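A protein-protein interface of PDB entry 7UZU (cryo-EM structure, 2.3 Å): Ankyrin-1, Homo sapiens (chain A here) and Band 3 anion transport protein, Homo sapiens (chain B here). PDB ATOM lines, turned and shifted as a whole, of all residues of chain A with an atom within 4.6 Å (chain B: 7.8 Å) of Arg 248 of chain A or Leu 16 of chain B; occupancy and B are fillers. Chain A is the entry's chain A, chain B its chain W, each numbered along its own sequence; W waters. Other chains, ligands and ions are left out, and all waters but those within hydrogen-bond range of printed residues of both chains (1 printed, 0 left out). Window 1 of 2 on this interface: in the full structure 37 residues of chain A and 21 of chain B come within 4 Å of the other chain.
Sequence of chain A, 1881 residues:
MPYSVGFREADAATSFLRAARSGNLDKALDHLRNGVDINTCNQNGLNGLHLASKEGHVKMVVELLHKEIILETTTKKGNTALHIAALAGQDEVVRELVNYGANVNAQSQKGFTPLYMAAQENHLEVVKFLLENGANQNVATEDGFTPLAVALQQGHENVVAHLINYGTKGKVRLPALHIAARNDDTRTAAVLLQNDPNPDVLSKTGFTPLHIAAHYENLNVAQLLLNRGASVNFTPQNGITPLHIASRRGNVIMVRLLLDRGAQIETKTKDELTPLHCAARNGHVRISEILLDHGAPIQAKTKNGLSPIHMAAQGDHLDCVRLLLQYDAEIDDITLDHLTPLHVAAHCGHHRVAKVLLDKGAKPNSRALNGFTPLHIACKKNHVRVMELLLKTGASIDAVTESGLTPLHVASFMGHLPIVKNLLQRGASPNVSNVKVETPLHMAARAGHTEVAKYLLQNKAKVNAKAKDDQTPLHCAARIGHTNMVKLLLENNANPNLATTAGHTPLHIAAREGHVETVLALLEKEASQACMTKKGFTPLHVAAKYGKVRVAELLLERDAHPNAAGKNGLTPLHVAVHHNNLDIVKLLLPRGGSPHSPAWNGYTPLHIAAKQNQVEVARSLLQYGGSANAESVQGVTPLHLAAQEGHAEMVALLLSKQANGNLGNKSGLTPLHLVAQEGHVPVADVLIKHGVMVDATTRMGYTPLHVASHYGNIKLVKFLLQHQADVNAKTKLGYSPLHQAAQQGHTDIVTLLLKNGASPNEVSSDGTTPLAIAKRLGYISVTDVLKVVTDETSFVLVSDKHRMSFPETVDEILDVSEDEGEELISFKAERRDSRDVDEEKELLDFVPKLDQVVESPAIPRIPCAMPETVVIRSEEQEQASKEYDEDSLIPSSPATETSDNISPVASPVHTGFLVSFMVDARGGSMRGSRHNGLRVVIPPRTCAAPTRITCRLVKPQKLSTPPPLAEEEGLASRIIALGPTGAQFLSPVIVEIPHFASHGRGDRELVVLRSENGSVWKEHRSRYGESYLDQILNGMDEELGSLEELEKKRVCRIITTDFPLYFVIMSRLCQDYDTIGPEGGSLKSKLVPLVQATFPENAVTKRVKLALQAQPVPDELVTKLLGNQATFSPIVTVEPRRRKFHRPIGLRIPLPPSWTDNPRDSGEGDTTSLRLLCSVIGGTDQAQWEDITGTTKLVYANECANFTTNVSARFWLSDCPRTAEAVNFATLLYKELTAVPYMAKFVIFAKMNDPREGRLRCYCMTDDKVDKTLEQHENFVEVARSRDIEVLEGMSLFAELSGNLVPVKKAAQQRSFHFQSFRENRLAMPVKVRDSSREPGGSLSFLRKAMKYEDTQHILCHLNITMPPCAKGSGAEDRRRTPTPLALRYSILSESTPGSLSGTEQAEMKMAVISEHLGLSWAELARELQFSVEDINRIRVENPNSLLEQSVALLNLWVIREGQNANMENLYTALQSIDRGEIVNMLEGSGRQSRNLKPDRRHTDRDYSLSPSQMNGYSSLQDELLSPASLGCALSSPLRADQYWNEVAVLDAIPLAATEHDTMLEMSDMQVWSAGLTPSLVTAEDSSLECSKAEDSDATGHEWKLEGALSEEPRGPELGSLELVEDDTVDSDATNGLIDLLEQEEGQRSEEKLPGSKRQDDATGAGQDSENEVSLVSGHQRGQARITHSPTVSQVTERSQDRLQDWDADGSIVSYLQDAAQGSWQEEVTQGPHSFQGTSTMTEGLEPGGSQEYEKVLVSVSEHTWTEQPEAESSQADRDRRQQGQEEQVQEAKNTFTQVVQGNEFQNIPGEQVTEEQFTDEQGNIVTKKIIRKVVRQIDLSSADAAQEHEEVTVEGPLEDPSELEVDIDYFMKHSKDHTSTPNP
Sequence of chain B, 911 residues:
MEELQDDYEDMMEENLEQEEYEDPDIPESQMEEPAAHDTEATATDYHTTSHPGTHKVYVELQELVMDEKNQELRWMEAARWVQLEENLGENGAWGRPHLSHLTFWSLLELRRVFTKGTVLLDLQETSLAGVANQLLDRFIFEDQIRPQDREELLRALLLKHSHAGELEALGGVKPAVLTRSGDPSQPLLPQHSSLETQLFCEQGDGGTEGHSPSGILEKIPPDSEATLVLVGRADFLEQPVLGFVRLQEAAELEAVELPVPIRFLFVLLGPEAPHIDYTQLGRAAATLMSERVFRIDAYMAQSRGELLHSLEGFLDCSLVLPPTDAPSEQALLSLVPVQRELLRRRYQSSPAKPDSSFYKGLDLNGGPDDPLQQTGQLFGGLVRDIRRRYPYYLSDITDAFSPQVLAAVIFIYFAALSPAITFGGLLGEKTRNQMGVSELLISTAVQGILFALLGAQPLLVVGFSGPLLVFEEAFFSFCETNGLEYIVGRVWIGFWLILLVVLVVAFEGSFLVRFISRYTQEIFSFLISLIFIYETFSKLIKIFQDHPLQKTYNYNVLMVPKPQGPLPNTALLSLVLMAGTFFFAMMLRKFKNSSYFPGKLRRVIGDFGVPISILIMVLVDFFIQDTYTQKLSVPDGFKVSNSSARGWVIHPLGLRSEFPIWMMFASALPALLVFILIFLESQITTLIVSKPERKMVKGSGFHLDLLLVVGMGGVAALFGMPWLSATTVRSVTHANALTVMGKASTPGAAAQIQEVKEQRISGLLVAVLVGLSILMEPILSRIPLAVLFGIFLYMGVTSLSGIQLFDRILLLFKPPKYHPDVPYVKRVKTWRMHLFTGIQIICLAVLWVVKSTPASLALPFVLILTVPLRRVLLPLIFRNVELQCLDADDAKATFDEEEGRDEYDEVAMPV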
ATOM      1  N   PHE A 207      -6.797 -18.050   3.916  1.00  0.00           N
ATOM      2  CA  PHE A 207      -6.560 -19.254   4.703  1.00  0.00           C
ATOM      3  C   PHE A 207      -6.038 -18.893   6.087  1.00  0.00           C
ATOM      4  O   PHE A 207      -5.244 -17.961   6.243  1.00  0.00           O
ATOM      5  CB  PHE A 207      -5.563 -20.170   3.992  1.00  0.00           C
ATOM      6  CG  PHE A 207      -6.129 -20.864   2.786  1.00  0.00           C
ATOM      7  CD1 PHE A 207      -7.102 -21.837   2.921  1.00  0.00           C
ATOM      8  CD2 PHE A 207      -5.694 -20.537   1.515  1.00  0.00           C
ATOM      9  CE1 PHE A 207      -7.625 -22.475   1.815  1.00  0.00           C
ATOM     10  CE2 PHE A 207      -6.214 -21.172   0.404  1.00  0.00           C
ATOM     11  CZ  PHE A 207      -7.181 -22.142   0.556  1.00  0.00           C
ATOM     12  N   ILE A 212      -2.800 -24.031   6.953  1.00  0.00           N
ATOM     13  CA  ILE A 212      -1.396 -24.306   6.661  1.00  0.00           C
ATOM     14  C   ILE A 212      -0.919 -25.517   7.453  1.00  0.00           C
ATOM     15  O   ILE A 212      -0.240 -26.402   6.921  1.00  0.00           O
ATOM     16  CB  ILE A 212      -0.533 -23.064   6.956  1.00  0.00           C
ATOM     17  CG1 ILE A 212      -1.049 -21.841   6.188  1.00  0.00           C
ATOM     18  CG2 ILE A 212       0.924 -23.337   6.622  1.00  0.00           C
ATOM     19  CD1 ILE A 212      -1.203 -22.045   4.698  1.00  0.00           C
ATOM     20  N   HIS A 215      -2.198 -28.617   5.856  1.00  0.00           N
ATOM     21  CA  HIS A 215      -1.533 -28.942   4.600  1.00  0.00           C
ATOM     22  C   HIS A 215      -0.225 -29.686   4.839  1.00  0.00           C
ATOM     23  O   HIS A 215       0.087 -30.646   4.127  1.00  0.00           O
ATOM     24  CB  HIS A 215      -1.289 -27.665   3.797  1.00  0.00           C
ATOM     25  CG  HIS A 215      -0.497 -27.878   2.546  1.00  0.00           C
ATOM     26  ND1 HIS A 215      -1.087 -28.080   1.317  1.00  0.00           N
ATOM     27  CD2 HIS A 215       0.838 -27.907   2.330  1.00  0.00           C
ATOM     28  CE1 HIS A 215      -0.149 -28.230   0.400  1.00  0.00           C
ATOM     29  NE2 HIS A 215       1.028 -28.131   0.989  1.00  0.00           N
ATOM     30  N   HIS A 244     -10.825 -30.610   4.438  1.00  0.00           N
ATOM     31  CA  HIS A 244     -10.613 -30.791   3.004  1.00  0.00           C
ATOM     32  C   HIS A 244      -9.129 -30.895   2.685  1.00  0.00           C
ATOM     33  O   HIS A 244      -8.700 -31.788   1.950  1.00  0.00           O
ATOM     34  CB  HIS A 244     -11.236 -29.630   2.225  1.00  0.00           C
ATOM     35  CG  HIS A 244     -12.712 -29.758   2.008  1.00  0.00           C
ATOM     36  ND1 HIS A 244     -13.637 -29.073   2.765  1.00  0.00           N
ATOM     37  CD2 HIS A 244     -13.421 -30.477   1.107  1.00  0.00           C
ATOM     38  CE1 HIS A 244     -14.853 -29.372   2.347  1.00  0.00           C
ATOM     39  NE2 HIS A 244     -14.750 -30.224   1.342  1.00  0.00           N
ATOM     40  N   ILE A 245      -8.329 -29.981   3.235  1.00  0.00           N
ATOM     41  CA  ILE A 245      -6.898 -29.979   2.944  1.00  0.00           C
ATOM     42  C   ILE A 245      -6.252 -31.257   3.461  1.00  0.00           C
ATOM     43  O   ILE A 245      -5.451 -31.895   2.767  1.00  0.00           O
ATOM     44  CB  ILE A 245      -6.232 -28.725   3.540  1.00  0.00           C
ATOM     45  CG1 ILE A 245      -6.631 -27.489   2.736  1.00  0.00           C
ATOM     46  CG2 ILE A 245      -4.719 -28.882   3.565  1.00  0.00           C
ATOM     47  CD1 ILE A 245      -6.259 -26.182   3.389  1.00  0.00           C
ATOM     48  N   ALA A 246      -6.596 -31.650   4.688  1.00  0.00           N
ATOM     49  CA  ALA A 246      -5.996 -32.846   5.268  1.00  0.00           C
ATOM     50  C   ALA A 246      -6.345 -34.086   4.453  1.00  0.00           C
ATOM     51  O   ALA A 246      -5.489 -34.945   4.224  1.00  0.00           O
ATOM     52  CB  ALA A 246      -6.445 -33.003   6.720  1.00  0.00           C
ATOM     53  N   SER A 247      -7.597 -34.194   4.001  1.00  0.00           N
ATOM     54  CA  SER A 247      -8.003 -35.355   3.215  1.00  0.00           C
ATOM     55  C   SER A 247      -7.353 -35.347   1.837  1.00  0.00           C
ATOM     56  O   SER A 247      -6.983 -36.404   1.316  1.00  0.00           O
ATOM     57  CB  SER A 247      -9.524 -35.400   3.084  1.00  0.00           C
ATOM     58  OG  SER A 247     -10.149 -34.961   4.273  1.00  0.00           O
ATOM     59  N   ARG A 248      -7.218 -34.170   1.226  1.00  0.00           N
ATOM     60  CA  ARG A 248      -6.577 -34.081  -0.082  1.00  0.00           C
ATOM     61  C   ARG A 248      -5.103 -34.452   0.002  1.00  0.00           C
ATOM     62  O   ARG A 248      -4.570 -35.116  -0.893  1.00  0.00           O
ATOM     63  CB  ARG A 248      -6.742 -32.670  -0.645  1.00  0.00           C
ATOM     64  CG  ARG A 248      -6.762 -32.588  -2.164  1.00  0.00           C
ATOM     65  CD  ARG A 248      -5.372 -32.464  -2.769  1.00  0.00           C
ATOM     66  NE  ARG A 248      -4.634 -31.313  -2.263  1.00  0.00           N
ATOM     67  CZ  ARG A 248      -3.498 -30.865  -2.777  1.00  0.00           C
ATOM     68  NH1 ARG A 248      -2.932 -31.447  -3.823  1.00  0.00           N
ATOM     69  NH2 ARG A 248      -2.915 -29.802  -2.233  1.00  0.00           N
ATOM     70  N   ARG A 249      -4.429 -34.030   1.072  1.00  0.00           N
ATOM     71  CA  ARG A 249      -2.998 -34.263   1.207  1.00  0.00           C
ATOM     72  C   ARG A 249      -2.667 -35.664   1.699  1.00  0.00           C
ATOM     73  O   ARG A 249      -1.494 -36.047   1.682  1.00  0.00           O
ATOM     74  CB  ARG A 249      -2.393 -33.234   2.163  1.00  0.00           C
ATOM     75  CG  ARG A 249      -2.436 -31.809   1.642  1.00  0.00           C
ATOM     76  CD  ARG A 249      -1.281 -31.520   0.705  1.00  0.00           C
ATOM     77  NE  ARG A 249      -0.004 -31.504   1.407  1.00  0.00           N
ATOM     78  CZ  ARG A 249       1.182 -31.459   0.816  1.00  0.00           C
ATOM     79  NH1 ARG A 249       1.299 -31.412  -0.502  1.00  0.00           N
ATOM     80  NH2 ARG A 249       2.280 -31.462   1.564  1.00  0.00           N
ATOM     81  N   GLY A 250      -3.659 -36.438   2.129  1.00  0.00           N
ATOM     82  CA  GLY A 250      -3.380 -37.750   2.674  1.00  0.00           C
ATOM     83  C   GLY A 250      -2.822 -37.728   4.077  1.00  0.00           C
ATOM     84  O   GLY A 250      -2.076 -38.635   4.452  1.00  0.00           O
ATOM     85  N   CYS A 278     -12.120 -35.353  -1.987  1.00  0.00           N
ATOM     86  CA  CYS A 278     -10.690 -35.065  -2.032  1.00  0.00           C
ATOM     87  C   CYS A 278      -9.864 -36.306  -1.724  1.00  0.00           C
ATOM     88  O   CYS A 278      -8.838 -36.547  -2.367  1.00  0.00           O
ATOM     89  CB  CYS A 278     -10.354 -33.940  -1.055  1.00  0.00           C
ATOM     90  SG  CYS A 278     -11.335 -32.441  -1.271  1.00  0.00           S
ATOM     91  N   ASN A 282      -7.376 -38.484  -4.772  1.00  0.00           N
ATOM     92  CA  ASN A 282      -5.949 -38.737  -4.633  1.00  0.00           C
ATOM     93  C   ASN A 282      -5.646 -40.143  -4.131  1.00  0.00           C
ATOM     94  O   ASN A 282      -4.496 -40.433  -3.788  1.00  0.00           O
ATOM     95  CB  ASN A 282      -5.328 -37.696  -3.703  1.00  0.00           C
ATOM     96  CG  ASN A 282      -5.464 -36.288  -4.238  1.00  0.00           C
ATOM     97  OD1 ASN A 282      -6.431 -35.590  -3.941  1.00  0.00           O
ATOM     98  ND2 ASN A 282      -4.499 -35.865  -5.039  1.00  0.00           N
ATOM     99  N   HIS A 284      -6.467 -41.911  -1.356  1.00  0.00           N
ATOM    100  CA  HIS A 284      -6.093 -42.078   0.047  1.00  0.00           C
ATOM    101  C   HIS A 284      -7.090 -43.037   0.686  1.00  0.00           C
ATOM    102  O   HIS A 284      -8.165 -42.632   1.131  1.00  0.00           O
ATOM    103  CB  HIS A 284      -6.057 -40.727   0.749  1.00  0.00           C
ATOM    104  CG  HIS A 284      -5.066 -39.774   0.161  1.00  0.00           C
ATOM    105  ND1 HIS A 284      -3.749 -40.114  -0.061  1.00  0.00           N
ATOM    106  CD2 HIS A 284      -5.199 -38.495  -0.257  1.00  0.00           C
ATOM    107  CE1 HIS A 284      -3.114 -39.084  -0.589  1.00  0.00           C
ATOM    108  NE2 HIS A 284      -3.971 -38.089  -0.718  1.00  0.00           N
ATOM    109  N   GLU B   9       3.173 -14.918   0.149  1.00  0.00           N
ATOM    110  CA  GLU B   9       1.774 -15.240  -0.113  1.00  0.00           C
ATOM    111  C   GLU B   9       1.595 -15.970  -1.439  1.00  0.00           C
ATOM    112  O   GLU B   9       0.818 -16.926  -1.521  1.00  0.00           O
ATOM    113  CB  GLU B   9       0.937 -13.964  -0.089  1.00  0.00           C
ATOM    114  CG  GLU B   9       0.833 -13.338   1.292  1.00  0.00           C
ATOM    115  CD  GLU B   9      -0.424 -13.748   2.035  1.00  0.00           C
ATOM    116  OE1 GLU B   9      -1.067 -14.738   1.629  1.00  0.00           O
ATOM    117  OE2 GLU B   9      -0.763 -13.086   3.039  1.00  0.00           O
ATOM    118  N   ASP B  10       2.286 -15.530  -2.492  1.00  0.00           N
ATOM    119  CA  ASP B  10       2.102 -16.152  -3.801  1.00  0.00           C
ATOM    120  C   ASP B  10       2.593 -17.594  -3.794  1.00  0.00           C
ATOM    121  O   ASP B  10       1.928 -18.500  -4.320  1.00  0.00           O
ATOM    122  CB  ASP B  10       2.831 -15.342  -4.871  1.00  0.00           C
ATOM    123  CG  ASP B  10       2.278 -13.939  -5.019  1.00  0.00           C
ATOM    124  OD1 ASP B  10       1.097 -13.722  -4.678  1.00  0.00           O
ATOM    125  OD2 ASP B  10       3.027 -13.055  -5.485  1.00  0.00           O
ATOM    126  N   MET B  11       3.763 -17.828  -3.197  1.00  0.00           N
ATOM    127  CA  MET B  11       4.290 -19.183  -3.123  1.00  0.00           C
ATOM    128  C   MET B  11       3.379 -20.077  -2.294  1.00  0.00           C
ATOM    129  O   MET B  11       3.166 -21.242  -2.638  1.00  0.00           O
ATOM    130  CB  MET B  11       5.705 -19.164  -2.538  1.00  0.00           C
ATOM    131  CG  MET B  11       6.497 -20.464  -2.695  1.00  0.00           C
ATOM    132  SD  MET B  11       6.642 -21.265  -4.323  1.00  0.00           S
ATOM    133  CE  MET B  11       6.306 -19.973  -5.527  1.00  0.00           C
ATOM    134  N   MET B  12       2.837 -19.553  -1.193  1.00  0.00           N
ATOM    135  CA  MET B  12       1.913 -20.349  -0.390  1.00  0.00           C
ATOM    136  C   MET B  12       0.640 -20.664  -1.164  1.00  0.00           C
ATOM    137  O   MET B  12       0.121 -21.784  -1.086  1.00  0.00           O
ATOM    138  CB  MET B  12       1.585 -19.622   0.915  1.00  0.00           C
ATOM    139  CG  MET B  12       0.906 -20.485   1.981  1.00  0.00           C
ATOM    140  SD  MET B  12       1.577 -22.149   2.179  1.00  0.00           S
ATOM    141  CE  MET B  12       2.958 -21.843   3.273  1.00  0.00           C
ATOM    142  N   GLU B  13       0.120 -19.693  -1.914  1.00  0.00           N
ATOM    143  CA  GLU B  13      -1.034 -19.956  -2.766  1.00  0.00           C
ATOM    144  C   GLU B  13      -0.747 -21.091  -3.736  1.00  0.00           C
ATOM    145  O   GLU B  13      -1.565 -22.002  -3.902  1.00  0.00           O
ATOM    146  CB  GLU B  13      -1.433 -18.695  -3.528  1.00  0.00           C
ATOM    147  CG  GLU B  13      -2.910 -18.635  -3.853  1.00  0.00           C
ATOM    148  CD  GLU B  13      -3.215 -17.694  -4.999  1.00  0.00           C
ATOM    149  OE1 GLU B  13      -2.394 -16.794  -5.266  1.00  0.00           O
ATOM    150  OE2 GLU B  13      -4.283 -17.849  -5.628  1.00  0.00           O
ATOM    151  N   GLU B  14       0.413 -21.051  -4.388  1.00  0.00           N
ATOM    152  CA  GLU B  14       0.764 -22.128  -5.306  1.00  0.00           C
ATOM    153  C   GLU B  14       0.914 -23.459  -4.579  1.00  0.00           C
ATOM    154  O   GLU B  14       0.519 -24.502  -5.109  1.00  0.00           O
ATOM    155  CB  GLU B  14       2.051 -21.781  -6.050  1.00  0.00           C
ATOM    156  CG  GLU B  14       1.863 -20.718  -7.111  1.00  0.00           C
ATOM    157  CD  GLU B  14       2.851 -20.850  -8.251  1.00  0.00           C
ATOM    158  OE1 GLU B  14       4.055 -21.032  -7.978  1.00  0.00           O
ATOM    159  OE2 GLU B  14       2.420 -20.771  -9.422  1.00  0.00           O
ATOM    160  N   ASN B  15       1.481 -23.443  -3.372  1.00  0.00           N
ATOM    161  CA  ASN B  15       1.698 -24.683  -2.636  1.00  0.00           C
ATOM    162  C   ASN B  15       0.378 -25.321  -2.217  1.00  0.00           C
ATOM    163  O   ASN B  15       0.238 -26.548  -2.257  1.00  0.00           O
ATOM    164  CB  ASN B  15       2.578 -24.417  -1.414  1.00  0.00           C
ATOM    165  CG  ASN B  15       4.045 -24.256  -1.773  1.00  0.00           C
ATOM    166  OD1 ASN B  15       4.576 -24.986  -2.609  1.00  0.00           O
ATOM    167  ND2 ASN B  15       4.708 -23.302  -1.134  1.00  0.00           N
ATOM    168  N   LEU B  16      -0.599 -24.508  -1.810  1.00  0.00           N
ATOM    169  CA  LEU B  16      -1.870 -25.044  -1.343  1.00  0.00           C
ATOM    170  C   LEU B  16      -2.746 -25.568  -2.475  1.00  0.00           C
ATOM    171  O   LEU B  16      -3.619 -26.403  -2.223  1.00  0.00           O
ATOM    172  CB  LEU B  16      -2.631 -23.980  -0.551  1.00  0.00           C
ATOM    173  CG  LEU B  16      -1.943 -23.487   0.724  1.00  0.00           C
ATOM    174  CD1 LEU B  16      -2.693 -22.303   1.308  1.00  0.00           C
ATOM    175  CD2 LEU B  16      -1.819 -24.602   1.752  1.00  0.00           C
ATOM    176  N   GLU B  17      -2.538 -25.097  -3.704  1.00  0.00           N
ATOM    177  CA  GLU B  17      -3.165 -25.673  -4.894  1.00  0.00           C
ATOM    178  C   GLU B  17      -4.693 -25.645  -4.799  1.00  0.00           C
ATOM    179  O   GLU B  17      -5.365 -26.673  -4.727  1.00  0.00           O
ATOM    180  CB  GLU B  17      -2.669 -27.104  -5.118  1.00  0.00           C
ATOM    181  CG  GLU B  17      -1.171 -27.225  -5.290  1.00  0.00           C
ATOM    182  CD  GLU B  17      -0.769 -28.521  -5.963  1.00  0.00           C
ATOM    183  OE1 GLU B  17      -0.220 -28.465  -7.083  1.00  0.00           O
ATOM    184  OE2 GLU B  17      -1.004 -29.596  -5.373  1.00  0.00           O
ATOM    185  N   GLN B  18      -5.230 -24.424  -4.806  1.00  0.00           N
ATOM    186  CA  GLN B  18      -6.682 -24.259  -4.783  1.00  0.00           C
ATOM    187  C   GLN B  18      -7.357 -25.005  -5.928  1.00  0.00           C
ATOM    188  O   GLN B  18      -8.507 -25.436  -5.795  1.00  0.00           O
ATOM    189  CB  GLN B  18      -7.044 -22.776  -4.848  1.00  0.00           C
ATOM    190  CG  GLN B  18      -6.814 -22.027  -3.546  1.00  0.00           C
ATOM    191  CD  GLN B  18      -6.122 -20.693  -3.743  1.00  0.00           C
ATOM    192  OE1 GLN B  18      -5.231 -20.327  -2.978  1.00  0.00           O
ATOM    193  NE2 GLN B  18      -6.544 -19.947  -4.758  1.00  0.00           N
ATOM    194  N   GLU B  19      -6.665 -25.165  -7.058  1.00  0.00           N
ATOM    195  CA  GLU B  19      -7.259 -25.829  -8.213  1.00  0.00           C
ATOM    196  C   GLU B  19      -7.559 -27.301  -7.955  1.00  0.00           C
ATOM    197  O   GLU B  19      -8.457 -27.856  -8.595  1.00  0.00           O
ATOM    198  CB  GLU B  19      -6.336 -25.694  -9.423  1.00  0.00           C
ATOM    199  N   GLU B  20      -6.837 -27.942  -7.039  1.00  0.00           N
ATOM    200  CA  GLU B  20      -7.043 -29.353  -6.740  1.00  0.00           C
ATOM    201  C   GLU B  20      -8.312 -29.617  -5.942  1.00  0.00           C
ATOM    202  O   GLU B  20      -8.664 -30.783  -5.743  1.00  0.00           O
ATOM    203  CB  GLU B  20      -5.836 -29.907  -5.974  1.00  0.00           C
ATOM    204  CG  GLU B  20      -4.542 -29.985  -6.783  1.00  0.00           C
ATOM    205  CD  GLU B  20      -4.716 -30.657  -8.132  1.00  0.00           C
ATOM    206  OE1 GLU B  20      -4.470 -29.997  -9.163  1.00  0.00           O
ATOM    207  OE2 GLU B  20      -5.099 -31.846  -8.162  1.00  0.00           O
ATOM    208  N   TYR B  21      -8.995 -28.574  -5.470  1.00  0.00           N
ATOM    209  CA  TYR B  21     -10.260 -28.717  -4.760  1.00  0.00           C
ATOM    210  C   TYR B  21     -11.448 -28.331  -5.631  1.00  0.00           C
ATOM    211  O   TYR B  21     -12.560 -28.171  -5.116  1.00  0.00           O
ATOM    212  CB  TYR B  21     -10.237 -27.879  -3.479  1.00  0.00           C
ATOM    213  CG  TYR B  21      -9.084 -28.243  -2.578  1.00  0.00           C
ATOM    214  CD1 TYR B  21      -7.832 -27.673  -2.758  1.00  0.00           C
ATOM    215  CD2 TYR B  21      -9.238 -29.179  -1.564  1.00  0.00           C
ATOM    216  CE1 TYR B  21      -6.772 -28.014  -1.950  1.00  0.00           C
ATOM    217  CE2 TYR B  21      -8.184 -29.523  -0.748  1.00  0.00           C
ATOM    218  CZ  TYR B  21      -6.952 -28.939  -0.946  1.00  0.00           C
ATOM    219  OH  TYR B  21      -5.894 -29.278  -0.140  1.00  0.00           O
HETATM  220  O   HOH W   1      -3.642 -28.196  -0.029  1.00  0.00           O
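Among the printed residues, pairs that only touch across the chains: His 215 of chain A with Asn 15 of chain B (3.2 Å), Ile 245 of chain A with Tyr 21 of chain B (3.3 Å), Phe 207 of chain A with Leu 16 of chain B (3.5 Å), His 244 of chain A with Tyr 21 of chain B (3.6 Å), His 215 of chain A with Leu 16 of chain B (3.6 Å), Phe 207 of chain A with Gln 18 of chain B (3.6 Å), Arg 248 of chain A with Glu 20 of chain B (3.7 Å), Ile 212 of chain A with Leu 16 of chain B (3.7 Å), Ile 212 of chain A with Met 12 of chain B (3.8 Å) and Cys 278 of chain A with Tyr 21 of chain B (3.9 Å).
Of chain B, only Leu 16 (3.5 Å), Glu 17 (3.1 Å), Glu 20 (3.7 Å) and Tyr 21 (3.2 Å) come within 4 Å of Arg 248 of chain A. Of the printed residues of chain A, Leu 16 of chain B touches Phe 207 (3.5 Å), Ile 212 (3.7 Å), His 215 (3.6 Å) and Arg 248 (3.5 Å). Of the printed residues of chain B, His 244 of chain A touches Tyr 21 (3.6 Å). Printed residues of chain B within 4 Å of Cys 278 of chain A: Tyr 21. Of the printed residues of chain A, Asn 15 of chain B touches His 215. Of the printed residues of chain A, Tyr 21 of chain B touches His 244 (3.6 Å), Ile 245 (3.3 Å), Arg 248 (3.2 Å) and Cys 278 (3.9 Å). Of the printed residues of chain B, His 215 of chain A touches Asn 15 and Leu 16. Ala 246 of chain A touches none of the printed residues of chain B. Gly 250 of chain A touches none of the printed residues of chain B. The nearest printed residue of chain A that does not touch Leu 16 of chain B is Ile 245 of chain A (5.0 Å). The nearest printed residue of chain B that does not touch His 244 of chain A is Glu 20 of chain B (7.8 Å).
Water W1 lies within hydrogen-bond range of the side-chain hydroxyl of Tyr 21 of chain B (2.5 Å), the guanidinium group of Arg 248 of chain A (2.8 Å), the backbone carbonyl oxygen of Leu 16 of chain B (2.8 Å) and a ring nitrogen (ND1) of His 215 of chain A (2.9 Å).
The backbone carbonyl oxygen (O) of His 215 of chain A lies within hydrogen-bond range of the guanidinium group (NE) of Arg 249 of chain A, 2.9 Å away. A ring nitrogen (NE2) of His 284 of chain A lies within hydrogen-bond range of the backbone carbonyl oxygen (O) of Arg 248 of chain A, 3.0 Å away. OD1 of Asn 282 of chain A sits close to O of Cys 278 of chain A (3.0 Å). The side-chain amide nitrogen (ND2) of Asn 15 of chain B lies within hydrogen-bond range of the backbone carbonyl oxygen (O) of Met 11 of chain B. The side-chain amide nitrogen of Gln 18 of chain B lies within hydrogen-bond range of the side-chain carboxylate of Glu 13 of chain B (3.2 Å).
The guanidinium group (NH2) of Arg 248 of chain A sits at hydrogen-bond distance from the backbone carbonyl oxygen (O) of Leu 16 of chain B (3.5 Å). The guanidinium group of Arg 248 of chain A is in salt-bridge range of the side-chain carboxylate of Glu 17 of chain B, at 3.1 Å. NE of Arg 248 of chain A sits at hydrogen-bond distance from OH of Tyr 21 of chain B, at 3.2 Å.
Of the 13 printed residues of chain B, 7 touch a printed residue of chain A. Printed residues of chain B that touch a printed residue of chain A: Met 12, Asn 15, Leu 16, Glu 17, Gln 18, Glu 20 and Tyr 21. Along chain B the printed residues that touch a printed residue of chain A span positions 12 to 21. Among the printed residues, Asp or Glu carboxylates within 4 Å of a Lys or Arg side-chain nitrogen of the other chain: Arg 248 of chain A with Glu 17 of chain B.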
